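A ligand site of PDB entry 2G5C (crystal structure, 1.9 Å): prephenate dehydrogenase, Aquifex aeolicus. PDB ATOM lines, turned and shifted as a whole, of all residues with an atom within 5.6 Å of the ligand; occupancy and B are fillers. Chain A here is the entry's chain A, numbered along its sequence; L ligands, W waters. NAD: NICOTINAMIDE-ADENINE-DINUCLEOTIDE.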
ATOM      1  N   VAL A   7       5.021  12.520  19.826  1.00  0.00           N
ATOM      2  CA  VAL A   7       5.203  11.423  20.783  1.00  0.00           C
ATOM      3  C   VAL A   7       4.136  10.396  20.467  1.00  0.00           C
ATOM      4  O   VAL A   7       2.945  10.639  20.658  1.00  0.00           O
ATOM      5  CB  VAL A   7       5.061  11.895  22.246  1.00  0.00           C
ATOM      6  CG1 VAL A   7       4.949  10.685  23.161  1.00  0.00           C
ATOM      7  CG2 VAL A   7       6.278  12.745  22.637  1.00  0.00           C
ATOM      8  N   GLY A   8       4.567   9.225  19.990  1.00  0.00           N
ATOM      9  CA  GLY A   8       3.633   8.187  19.602  1.00  0.00           C
ATOM     10  C   GLY A   8       3.365   8.407  18.128  1.00  0.00           C
ATOM     11  O   GLY A   8       2.432   9.126  17.746  1.00  0.00           O
ATOM     12  N   VAL A   9       4.192   7.807  17.277  1.00  0.00           N
ATOM     13  CA  VAL A   9       4.048   7.958  15.840  1.00  0.00           C
ATOM     14  C   VAL A   9       3.149   6.880  15.245  1.00  0.00           C
ATOM     15  O   VAL A   9       3.628   5.913  14.649  1.00  0.00           O
ATOM     16  CB  VAL A   9       5.427   7.914  15.130  1.00  0.00           C
ATOM     17  CG1 VAL A   9       5.279   8.348  13.681  1.00  0.00           C
ATOM     18  CG2 VAL A   9       6.414   8.820  15.850  1.00  0.00           C
ATOM     19  N   GLY A  10       1.846   7.051  15.435  1.00  0.00           N
ATOM     20  CA  GLY A  10       0.885   6.099  14.908  1.00  0.00           C
ATOM     21  C   GLY A  10      -0.050   6.774  13.936  1.00  0.00           C
ATOM     22  O   GLY A  10       0.346   7.713  13.222  1.00  0.00           O
ATOM     23  N   PHE A  11      -1.293   6.327  13.895  1.00  0.00           N
ATOM     24  CA  PHE A  11      -2.290   6.901  13.010  1.00  0.00           C
ATOM     25  C   PHE A  11      -2.502   8.392  13.295  1.00  0.00           C
ATOM     26  O   PHE A  11      -2.448   9.212  12.383  1.00  0.00           O
ATOM     27  CB  PHE A  11      -3.617   6.153  13.149  1.00  0.00           C
ATOM     28  CG  PHE A  11      -4.756   6.799  12.424  1.00  0.00           C
ATOM     29  CD1 PHE A  11      -4.752   6.875  11.038  1.00  0.00           C
ATOM     30  CD2 PHE A  11      -5.825   7.352  13.122  1.00  0.00           C
ATOM     31  CE1 PHE A  11      -5.799   7.498  10.348  1.00  0.00           C
ATOM     32  CE2 PHE A  11      -6.872   7.972  12.445  1.00  0.00           C
ATOM     33  CZ  PHE A  11      -6.851   8.042  11.058  1.00  0.00           C
ATOM     34  N   MET A  12      -2.750   8.724  14.549  1.00  0.00           N
ATOM     35  CA  MET A  12      -2.987  10.112  14.930  1.00  0.00           C
ATOM     36  C   MET A  12      -1.703  10.944  14.900  1.00  0.00           C
ATOM     37  O   MET A  12      -1.676  12.029  14.315  1.00  0.00           O
ATOM     38  CB  MET A  12      -3.631  10.170  16.322  1.00  0.00           C
ATOM     39  CG  MET A  12      -4.969   9.415  16.422  1.00  0.00           C
ATOM     40  SD  MET A  12      -6.385  10.144  15.307  1.00  0.00           S
ATOM     41  CE  MET A  12      -6.753  11.742  16.327  1.00  0.00           C
ATOM     42  N   GLY A  13      -0.657  10.446  15.544  1.00  0.00           N
ATOM     43  CA  GLY A  13       0.600  11.176  15.559  1.00  0.00           C
ATOM     44  C   GLY A  13       1.029  11.435  14.127  1.00  0.00           C
ATOM     45  O   GLY A  13       1.396  12.543  13.758  1.00  0.00           O
ATOM     46  N   TYR A  32       9.090  10.253  18.650  1.00  0.00           N
ATOM     47  CA  TYR A  32       9.520   9.398  19.746  1.00  0.00           C
ATOM     48  C   TYR A  32       8.471   8.300  19.851  1.00  0.00           C
ATOM     49  O   TYR A  32       7.279   8.588  19.960  1.00  0.00           O
ATOM     50  CB  TYR A  32       9.591  10.146  21.072  1.00  0.00           C
ATOM     51  CG  TYR A  32       9.674   9.212  22.266  1.00  0.00           C
ATOM     52  CD1 TYR A  32      10.735   8.309  22.398  1.00  0.00           C
ATOM     53  CD2 TYR A  32       8.662   9.177  23.217  1.00  0.00           C
ATOM     54  CE1 TYR A  32      10.773   7.396  23.450  1.00  0.00           C
ATOM     55  CE2 TYR A  32       8.689   8.262  24.276  1.00  0.00           C
ATOM     56  CZ  TYR A  32       9.751   7.383  24.384  1.00  0.00           C
ATOM     57  OH  TYR A  32       9.766   6.461  25.404  1.00  0.00           O
ATOM     58  N   ASP A  33       8.916   7.056  19.817  1.00  0.00           N
ATOM     59  CA  ASP A  33       8.018   5.922  19.896  1.00  0.00           C
ATOM     60  C   ASP A  33       8.805   4.745  20.449  1.00  0.00           C
ATOM     61  O   ASP A  33      10.008   4.630  20.205  1.00  0.00           O
ATOM     62  CB  ASP A  33       7.507   5.587  18.490  1.00  0.00           C
ATOM     63  CG  ASP A  33       6.240   4.770  18.509  1.00  0.00           C
ATOM     64  OD1 ASP A  33       6.278   3.608  18.981  1.00  0.00           O
ATOM     65  OD2 ASP A  33       5.196   5.292  18.063  1.00  0.00           O
ATOM     66  N   ILE A  34       8.147   3.875  21.202  1.00  0.00           N
ATOM     67  CA  ILE A  34       8.810   2.713  21.769  1.00  0.00           C
ATOM     68  C   ILE A  34       9.020   1.642  20.703  1.00  0.00           C
ATOM     69  O   ILE A  34       9.767   0.686  20.926  1.00  0.00           O
ATOM     70  CB  ILE A  34       7.992   2.069  22.907  1.00  0.00           C
ATOM     71  CG1 ILE A  34       6.581   1.744  22.417  1.00  0.00           C
ATOM     72  CG2 ILE A  34       7.983   2.994  24.109  1.00  0.00           C
ATOM     73  CD1 ILE A  34       5.766   0.899  23.368  1.00  0.00           C
ATOM     74  N   ASN A  35       8.357   1.799  19.564  1.00  0.00           N
ATOM     75  CA  ASN A  35       8.471   0.821  18.490  1.00  0.00           C
ATOM     76  C   ASN A  35       9.411   1.286  17.389  1.00  0.00           C
ATOM     77  O   ASN A  35       9.166   2.293  16.722  1.00  0.00           O
ATOM     78  CB  ASN A  35       7.092   0.534  17.901  1.00  0.00           C
ATOM     79  CG  ASN A  35       7.156  -0.331  16.651  1.00  0.00           C
ATOM     80  OD1 ASN A  35       7.641  -1.458  16.694  1.00  0.00           O
ATOM     81  ND2 ASN A  35       6.677   0.202  15.532  1.00  0.00           N
ATOM     82  N   SER A  38       7.895   1.976  13.922  1.00  0.00           N
ATOM     83  CA  SER A  38       7.104   3.205  13.794  1.00  0.00           C
ATOM     84  C   SER A  38       7.999   4.335  13.288  1.00  0.00           C
ATOM     85  O   SER A  38       7.630   5.075  12.375  1.00  0.00           O
ATOM     86  CB  SER A  38       6.498   3.586  15.142  1.00  0.00           C
ATOM     87  OG  SER A  38       5.706   2.534  15.665  1.00  0.00           O
ATOM     88  N   SER A  69       0.705  11.768  21.330  1.00  0.00           N
ATOM     89  CA  SER A  69      -0.169  10.994  20.473  1.00  0.00           C
ATOM     90  C   SER A  69      -0.036   9.500  20.734  1.00  0.00           C
ATOM     91  O   SER A  69      -0.314   8.680  19.857  1.00  0.00           O
ATOM     92  CB  SER A  69       0.160  11.303  19.015  1.00  0.00           C
ATOM     93  OG  SER A  69       0.260  12.700  18.824  1.00  0.00           O
ATOM     94  N   SER A  70       0.394   9.161  21.933  1.00  0.00           N
ATOM     95  CA  SER A  70       0.549   7.770  22.340  1.00  0.00           C
ATOM     96  C   SER A  70      -0.665   7.423  23.206  1.00  0.00           C
ATOM     97  O   SER A  70      -1.545   8.263  23.394  1.00  0.00           O
ATOM     98  CB  SER A  70       1.844   7.615  23.151  1.00  0.00           C
ATOM     99  OG  SER A  70       1.880   8.529  24.235  1.00  0.00           O
ATOM    100  N   PRO A  71      -0.744   6.186  23.712  1.00  0.00           N
ATOM    101  CA  PRO A  71      -1.903   5.859  24.550  1.00  0.00           C
ATOM    102  C   PRO A  71      -1.975   6.756  25.793  1.00  0.00           C
ATOM    103  O   PRO A  71      -0.956   7.063  26.404  1.00  0.00           O
ATOM    104  CB  PRO A  71      -1.658   4.389  24.894  1.00  0.00           C
ATOM    105  CG  PRO A  71      -1.008   3.878  23.629  1.00  0.00           C
ATOM    106  CD  PRO A  71      -0.006   4.983  23.326  1.00  0.00           C
ATOM    107  N   VAL A  72      -3.177   7.181  26.151  1.00  0.00           N
ATOM    108  CA  VAL A  72      -3.336   8.052  27.311  1.00  0.00           C
ATOM    109  C   VAL A  72      -2.670   7.470  28.563  1.00  0.00           C
ATOM    110  O   VAL A  72      -2.184   8.205  29.417  1.00  0.00           O
ATOM    111  CB  VAL A  72      -4.837   8.321  27.608  1.00  0.00           C
ATOM    112  CG1 VAL A  72      -4.994   8.974  28.981  1.00  0.00           C
ATOM    113  CG2 VAL A  72      -5.402   9.257  26.551  1.00  0.00           C
ATOM    114  N   THR A  74       0.062   6.257  28.810  1.00  0.00           N
ATOM    115  CA  THR A  74       1.489   6.594  28.791  1.00  0.00           C
ATOM    116  C   THR A  74       1.813   8.062  29.038  1.00  0.00           C
ATOM    117  O   THR A  74       2.967   8.421  29.257  1.00  0.00           O
ATOM    118  CB  THR A  74       2.143   6.192  27.453  1.00  0.00           C
ATOM    119  OG1 THR A  74       1.613   7.004  26.385  1.00  0.00           O
ATOM    120  CG2 THR A  74       1.878   4.727  27.150  1.00  0.00           C
ATOM    121  N   PHE A  75       0.793   8.909  29.003  1.00  0.00           N
ATOM    122  CA  PHE A  75       0.984  10.339  29.198  1.00  0.00           C
ATOM    123  C   PHE A  75       1.683  10.718  30.499  1.00  0.00           C
ATOM    124  O   PHE A  75       2.658  11.458  30.485  1.00  0.00           O
ATOM    125  CB  PHE A  75      -0.363  11.055  29.102  1.00  0.00           C
ATOM    126  CG  PHE A  75      -0.913  11.144  27.699  1.00  0.00           C
ATOM    127  CD1 PHE A  75      -0.498  10.256  26.704  1.00  0.00           C
ATOM    128  CD2 PHE A  75      -1.873  12.105  27.374  1.00  0.00           C
ATOM    129  CE1 PHE A  75      -1.028  10.316  25.411  1.00  0.00           C
ATOM    130  CE2 PHE A  75      -2.403  12.182  26.086  1.00  0.00           C
ATOM    131  CZ  PHE A  75      -1.984  11.282  25.110  1.00  0.00           C
ATOM    132  N   GLU A  77       3.600   8.975  32.589  1.00  0.00           N
ATOM    133  CA  GLU A  77       4.984   8.508  32.652  1.00  0.00           C
ATOM    134  C   GLU A  77       5.904   9.312  31.737  1.00  0.00           C
ATOM    135  O   GLU A  77       7.016   9.678  32.125  1.00  0.00           O
ATOM    136  CB  GLU A  77       5.065   7.026  32.269  1.00  0.00           C
ATOM    137  CG  GLU A  77       4.417   6.710  30.929  1.00  0.00           C
ATOM    138  CD  GLU A  77       4.555   5.257  30.527  1.00  0.00           C
ATOM    139  OE1 GLU A  77       5.669   4.850  30.127  1.00  0.00           O
ATOM    140  OE2 GLU A  77       3.553   4.512  30.626  1.00  0.00           O
ATOM    141  N   ILE A  78       5.436   9.582  30.525  1.00  0.00           N
ATOM    142  CA  ILE A  78       6.209  10.349  29.551  1.00  0.00           C
ATOM    143  C   ILE A  78       6.376  11.809  29.988  1.00  0.00           C
ATOM    144  O   ILE A  78       7.467  12.389  29.876  1.00  0.00           O
ATOM    145  CB  ILE A  78       5.543  10.301  28.151  1.00  0.00           C
ATOM    146  CG1 ILE A  78       5.443   8.846  27.673  1.00  0.00           C
ATOM    147  CG2 ILE A  78       6.338  11.117  27.154  1.00  0.00           C
ATOM    148  CD1 ILE A  78       4.736   8.691  26.338  1.00  0.00           C
ATOM    149  N   GLN A  95      -3.610  14.621  22.179  1.00  0.00           N
ATOM    150  CA  GLN A  95      -4.708  14.184  21.318  1.00  0.00           C
ATOM    151  C   GLN A  95      -5.568  13.167  22.046  1.00  0.00           C
ATOM    152  O   GLN A  95      -6.538  12.642  21.488  1.00  0.00           O
ATOM    153  CB  GLN A  95      -4.146  13.532  20.048  1.00  0.00           C
ATOM    154  CG  GLN A  95      -3.512  14.492  19.070  1.00  0.00           C
ATOM    155  CD  GLN A  95      -3.262  13.859  17.713  1.00  0.00           C
ATOM    156  OE1 GLN A  95      -2.209  13.271  17.475  1.00  0.00           O
ATOM    157  NE2 GLN A  95      -4.236  13.981  16.817  1.00  0.00           N
ATOM    158  N   GLY A  96      -5.220  12.880  23.300  1.00  0.00           N
ATOM    159  CA  GLY A  96      -5.962  11.921  24.099  1.00  0.00           C
ATOM    160  C   GLY A  96      -7.468  12.041  23.975  1.00  0.00           C
ATOM    161  O   GLY A  96      -7.995  13.146  23.858  1.00  0.00           O
ATOM    162  N   SER A  97      -8.164  10.911  24.011  1.00  0.00           N
ATOM    163  CA  SER A  97      -9.619  10.862  23.894  1.00  0.00           C
ATOM    164  C   SER A  97     -10.287  11.318  25.187  1.00  0.00           C
ATOM    165  O   SER A  97     -11.458  11.701  25.190  1.00  0.00           O
ATOM    166  CB  SER A  97     -10.095   9.446  23.567  1.00  0.00           C
ATOM    167  OG  SER A  97      -9.620   9.012  22.309  1.00  0.00           O
ATOM    168  N   VAL A  98      -9.543  11.238  26.285  1.00  0.00           N
ATOM    169  CA  VAL A  98     -10.069  11.645  27.578  1.00  0.00           C
ATOM    170  C   VAL A  98      -9.268  12.834  28.118  1.00  0.00           C
ATOM    171  O   VAL A  98      -8.095  13.005  27.811  1.00  0.00           O
ATOM    172  CB  VAL A  98     -10.005  10.496  28.618  1.00  0.00           C
ATOM    173  CG1 VAL A  98     -10.824   9.298  28.133  1.00  0.00           C
ATOM    174  CG2 VAL A  98      -8.564  10.085  28.867  1.00  0.00           C
ATOM    175  N   HIS A 118      -8.210  17.552  22.234  1.00  0.00           N
ATOM    176  CA  HIS A 118      -8.869  16.337  21.743  1.00  0.00           C
ATOM    177  C   HIS A 118      -9.517  16.558  20.387  1.00  0.00           C
ATOM    178  O   HIS A 118     -10.588  17.168  20.301  1.00  0.00           O
ATOM    179  CB  HIS A 118      -9.945  15.876  22.723  1.00  0.00           C
ATOM    180  CG  HIS A 118     -10.743  14.705  22.224  1.00  0.00           C
ATOM    181  ND1 HIS A 118     -11.951  14.340  22.785  1.00  0.00           N
ATOM    182  CD2 HIS A 118     -10.515  13.826  21.225  1.00  0.00           C
ATOM    183  CE1 HIS A 118     -12.428  13.283  22.145  1.00  0.00           C
ATOM    184  NE2 HIS A 118     -11.573  12.948  21.199  1.00  0.00           N
ATOM    185  N   PRO A 119      -8.885  16.068  19.310  1.00  0.00           N
ATOM    186  CA  PRO A 119      -9.436  16.214  17.966  1.00  0.00           C
ATOM    187  C   PRO A 119     -10.536  15.179  17.771  1.00  0.00           C
ATOM    188  O   PRO A 119     -10.343  13.997  18.089  1.00  0.00           O
ATOM    189  CB  PRO A 119      -8.235  15.963  17.077  1.00  0.00           C
ATOM    190  CG  PRO A 119      -7.471  14.927  17.858  1.00  0.00           C
ATOM    191  CD  PRO A 119      -7.528  15.493  19.262  1.00  0.00           C
ATOM    192  N   ALA A 121     -11.789  13.312  15.368  1.00  0.00           N
ATOM    193  CA  ALA A 121     -11.601  12.720  14.056  1.00  0.00           C
ATOM    194  C   ALA A 121     -10.928  11.363  14.220  1.00  0.00           C
ATOM    195  O   ALA A 121     -10.729  10.886  15.336  1.00  0.00           O
ATOM    196  CB  ALA A 121     -10.743  13.637  13.192  1.00  0.00           C
ATOM    197  N   GLY A 122     -10.566  10.743  13.098  1.00  0.00           N
ATOM    198  CA  GLY A 122      -9.916   9.442  13.136  1.00  0.00           C
ATOM    199  C   GLY A 122     -10.902   8.300  13.026  1.00  0.00           C
ATOM    200  O   GLY A 122     -11.745   8.109  13.905  1.00  0.00           O
ATOM    201  N   THR A 123     -10.796   7.539  11.945  1.00  0.00           N
ATOM    202  CA  THR A 123     -11.692   6.410  11.718  1.00  0.00           C
ATOM    203  C   THR A 123     -11.278   5.181  12.515  1.00  0.00           C
ATOM    204  O   THR A 123     -11.440   4.048  12.063  1.00  0.00           O
ATOM    205  CB  THR A 123     -11.756   6.037  10.222  1.00  0.00           C
ATOM    206  OG1 THR A 123     -10.434   5.742   9.758  1.00  0.00           O
ATOM    207  CG2 THR A 123     -12.322   7.188   9.406  1.00  0.00           C
ATOM    208  N   GLU A 124     -10.754   5.414  13.718  1.00  0.00           N
ATOM    209  CA  GLU A 124     -10.316   4.341  14.602  1.00  0.00           C
ATOM    210  C   GLU A 124      -9.139   3.514  14.076  1.00  0.00           C
ATOM    211  O   GLU A 124      -8.598   2.686  14.803  1.00  0.00           O
ATOM    212  CB  GLU A 124     -11.487   3.397  14.913  1.00  0.00           C
ATOM    213  CG  GLU A 124     -12.650   4.038  15.667  1.00  0.00           C
ATOM    214  CD  GLU A 124     -13.487   4.968  14.811  1.00  0.00           C
ATOM    215  OE1 GLU A 124     -14.046   4.505  13.793  1.00  0.00           O
ATOM    216  OE2 GLU A 124     -13.583   6.173  15.155  1.00  0.00           O
ATOM    217  N   LYS A 125      -8.744   3.746  12.834  1.00  0.00           N
ATOM    218  CA  LYS A 125      -7.633   3.004  12.234  1.00  0.00           C
ATOM    219  C   LYS A 125      -6.408   3.015  13.138  1.00  0.00           C
ATOM    220  O   LYS A 125      -6.245   3.915  13.966  1.00  0.00           O
ATOM    221  CB  LYS A 125      -7.270   3.582  10.864  1.00  0.00           C
ATOM    222  CG  LYS A 125      -8.386   3.500   9.841  1.00  0.00           C
ATOM    223  CD  LYS A 125      -7.884   3.788   8.435  1.00  0.00           C
ATOM    224  CE  LYS A 125      -7.299   5.190   8.300  1.00  0.00           C
ATOM    225  NZ  LYS A 125      -8.312   6.251   8.535  1.00  0.00           N
ATOM    226  N   SER A 126      -5.543   2.025  12.975  1.00  0.00           N
ATOM    227  CA  SER A 126      -4.336   1.931  13.785  1.00  0.00           C
ATOM    228  C   SER A 126      -3.095   1.716  12.936  1.00  0.00           C
ATOM    229  O   SER A 126      -3.083   0.870  12.041  1.00  0.00           O
ATOM    230  CB  SER A 126      -4.467   0.788  14.805  1.00  0.00           C
ATOM    231  OG  SER A 126      -3.352   0.756  15.672  1.00  0.00           O
ATOM    232  N   GLY A 127      -2.043   2.483  13.218  1.00  0.00           N
ATOM    233  CA  GLY A 127      -0.811   2.362  12.467  1.00  0.00           C
ATOM    234  C   GLY A 127      -0.502   3.635  11.686  1.00  0.00           C
ATOM    235  O   GLY A 127      -1.384   4.186  11.019  1.00  0.00           O
ATOM    236  N   VAL A 128       0.739   4.089  11.773  1.00  0.00           N
ATOM    237  CA  VAL A 128       1.167   5.302  11.083  1.00  0.00           C
ATOM    238  C   VAL A 128       1.005   5.137   9.574  1.00  0.00           C
ATOM    239  O   VAL A 128       0.990   6.114   8.833  1.00  0.00           O
ATOM    240  CB  VAL A 128       2.649   5.628  11.415  1.00  0.00           C
ATOM    241  CG1 VAL A 128       3.532   4.474  10.995  1.00  0.00           C
ATOM    242  CG2 VAL A 128       3.070   6.909  10.713  1.00  0.00           C
ATOM    243  N   MET A 229      -7.648   0.155  24.143  1.00  0.00           N
ATOM    244  CA  MET A 229      -7.973   1.584  24.239  1.00  0.00           C
ATOM    245  C   MET A 229      -9.246   1.788  25.039  1.00  0.00           C
ATOM    246  O   MET A 229      -9.299   2.620  25.944  1.00  0.00           O
ATOM    247  CB  MET A 229      -8.160   2.192  22.835  1.00  0.00           C
ATOM    248  CG  MET A 229      -8.527   3.687  22.867  1.00  0.00           C
ATOM    249  SD  MET A 229      -8.753   4.503  21.115  1.00  0.00           S
ATOM    250  CE  MET A 229     -10.678   4.414  20.977  1.00  0.00           C
HETATM  251  PA  NAD L   1      -1.839   3.923  17.220  1.00  0.00           P
HETATM  252  O1A NAD L   1      -1.970   4.062  15.758  1.00  0.00           O
HETATM  253  O2A NAD L   1      -1.886   2.515  17.761  1.00  0.00           O
HETATM  254  O5B NAD L   1      -0.485   4.658  17.614  1.00  0.00           O
HETATM  255  C5B NAD L   1      -0.066   4.695  18.951  1.00  0.00           C
HETATM  256  C4B NAD L   1       1.445   4.791  19.002  1.00  0.00           C
HETATM  257  O4B NAD L   1       1.765   4.768  20.363  1.00  0.00           O
HETATM  258  C3B NAD L   1       2.154   3.562  18.380  1.00  0.00           C
HETATM  259  O3B NAD L   1       3.007   3.915  17.297  1.00  0.00           O
HETATM  260  C2B NAD L   1       2.870   2.940  19.579  1.00  0.00           C
HETATM  261  O2B NAD L   1       4.078   2.259  19.307  1.00  0.00           O
HETATM  262  C1B NAD L   1       3.024   4.170  20.445  1.00  0.00           C
HETATM  263  N9A NAD L   1       3.327   4.020  21.881  1.00  0.00           N
HETATM  264  C8A NAD L   1       2.819   3.130  22.795  1.00  0.00           C
HETATM  265  N7A NAD L   1       3.385   3.361  23.984  1.00  0.00           N
HETATM  266  C5A NAD L   1       4.262   4.378  23.851  1.00  0.00           C
HETATM  267  C6A NAD L   1       5.138   5.050  24.731  1.00  0.00           C
HETATM  268  N6A NAD L   1       5.215   4.706  26.004  1.00  0.00           N
HETATM  269  N1A NAD L   1       5.924   6.095  24.257  1.00  0.00           N
HETATM  270  C2A NAD L   1       5.863   6.476  22.914  1.00  0.00           C
HETATM  271  N3A NAD L   1       5.011   5.821  22.040  1.00  0.00           N
HETATM  272  C4A NAD L   1       4.233   4.798  22.520  1.00  0.00           C
HETATM  273  O3  NAD L   1      -2.971   4.797  18.016  1.00  0.00           O
HETATM  274  PN  NAD L   1      -3.727   6.098  17.447  1.00  0.00           P
HETATM  275  O1N NAD L   1      -2.781   6.860  16.602  1.00  0.00           O
HETATM  276  O2N NAD L   1      -4.983   5.650  16.789  1.00  0.00           O
HETATM  277  O5D NAD L   1      -4.167   6.989  18.719  1.00  0.00           O
HETATM  278  C5D NAD L   1      -3.210   7.582  19.581  1.00  0.00           C
HETATM  279  C4D NAD L   1      -3.851   8.492  20.654  1.00  0.00           C
HETATM  280  O4D NAD L   1      -4.846   9.317  20.057  1.00  0.00           O
HETATM  281  C3D NAD L   1      -4.525   7.827  21.865  1.00  0.00           C
HETATM  282  O3D NAD L   1      -4.043   8.442  23.052  1.00  0.00           O
HETATM  283  C2D NAD L   1      -6.015   8.051  21.688  1.00  0.00           C
HETATM  284  O2D NAD L   1      -6.710   8.219  22.918  1.00  0.00           O
HETATM  285  C1D NAD L   1      -6.058   9.274  20.771  1.00  0.00           C
HETATM  286  N1N NAD L   1      -7.177   9.334  19.780  1.00  0.00           N
HETATM  287  C2N NAD L   1      -7.370   8.247  18.937  1.00  0.00           C
HETATM  288  C3N NAD L   1      -8.414   8.271  17.989  1.00  0.00           C
HETATM  289  C7N NAD L   1      -8.602   7.087  17.084  1.00  0.00           C
HETATM  290  O7N NAD L   1      -9.627   7.140  16.182  1.00  0.00           O
HETATM  291  N7N NAD L   1      -7.839   6.002  17.119  1.00  0.00           N
HETATM  292  C4N NAD L   1      -9.253   9.408  17.915  1.00  0.00           C
HETATM  293  C5N NAD L   1      -9.044  10.519  18.779  1.00  0.00           C
HETATM  294  C6N NAD L   1      -8.000  10.462  19.718  1.00  0.00           C
HETATM  295  O   HOH W   1     -12.169  10.928  19.503  1.00  0.00           O
HETATM  296  O   HOH W   2      -0.402   8.140  17.011  1.00  0.00           O
HETATM  297  O   HOH W   3      -7.460   6.495  25.774  1.00  0.00           O
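O of Ser 70 lies within hydrogen-bond range of O3D of the ligand (2.5 Å).
O2B of the ligand sits at hydrogen-bond distance from OD1 of Asp 33, at 2.6 Å.
The backbone NH of Met 12 is in hydrogen-bond range of an oxygen (O1N) of the ligand, at 2.8 Å.
The backbone NH (N) of Gly 127 sits at hydrogen-bond distance from an oxygen (O1A) of the ligand, 3.0 Å away.
An oxygen (O1A) of the ligand sits at hydrogen-bond distance from the backbone NH (N) of Phe 11 (3.0 Å).
The backbone NH (N) of Ser 97 lies within hydrogen-bond range of an oxygen (O2D) of the ligand (3.2 Å).
The side-chain hydroxyl of Ser 97 sits at hydrogen-bond distance from an oxygen (O2D) of the ligand, at 3.1 Å.
OG of Ser 126 sits at hydrogen-bond distance from O2A of the ligand (3.1 Å).
N of Glu 124 lies within hydrogen-bond range of O7N of the ligand (3.2 Å).
The backbone carbonyl oxygen of Val 9 sits at hydrogen-bond distance from an oxygen (O3B) of the ligand (3.4 Å).
O3B of the ligand is in hydrogen-bond range of OG of Ser 38, 3.4 Å away.
The backbone NH (N) of Val 72 lies within hydrogen-bond range of an oxygen (O3D) of the ligand, 3.5 Å away.
The side-chain hydroxyl of Ser 70 is in hydrogen-bond range of the side-chain hydroxyl of Thr 74, at 2.6 Å.
The side-chain carboxylate of Asp 33 lies within hydrogen-bond range of the backbone NH of Val 9 (2.8 Å).
The backbone carbonyl oxygen (O) of Met 12 lies close to the side-chain amide oxygen (OE1) of Gln 95.
The side-chain hydroxyl (OG) of Ser 69 sits at hydrogen-bond distance from the side-chain amide oxygen (OE1) of Gln 95, at 2.9 Å.
N of Ser 69 sits at hydrogen-bond distance from O of Val 7 (2.6 Å).
The backbone carbonyl oxygen (O) of Pro 71 sits at hydrogen-bond distance from the side-chain hydroxyl (OG1) of Thr 74.
The side-chain hydroxyl (OG) of Ser 38 is in hydrogen-bond range of the side-chain amide nitrogen (ND2) of Asn 35 (2.5 Å).
N of Gly 8 is in hydrogen-bond range of O of Tyr 32 (2.8 Å).
An oxygen (O7N) of the ligand sits close to the backbone carbonyl oxygen (O) of Gly 122 (3.3 Å).
Gly 8 touches the ligand.
CA of Gly 10 touches O5B of the ligand, at 3.4 Å.
Tyr 32 touches the ligand (CE2 to N1A, 3.5 Å).
Ile 34 touches the ligand.
Asn 35 touches the ligand (CB to O2B, 3.7 Å).
Ser 69 touches the ligand.
Pro 71 touches the ligand (CD to C8A, 3.4 Å).
Thr 74 touches the ligand.
CD1 of Ile 78 touches N1A of the ligand (3.5 Å).
Gln 95 touches the ligand.
Gly 96 touches the ligand.
Pro 119 touches the ligand.
Ala 121 touches the ligand (O to C4N, 3.3 Å).
O of Lys 125 touches O2N of the ligand (3.5 Å).
Hydrophobic or aromatic side chains within 4 Å of the ligand: Phe 11, Met 12, Tyr 32, Ile 34, Pro 71, Val 72 and Ile 78.
Of the 35 residues printed, 26 come within 4 Å of the ligand.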
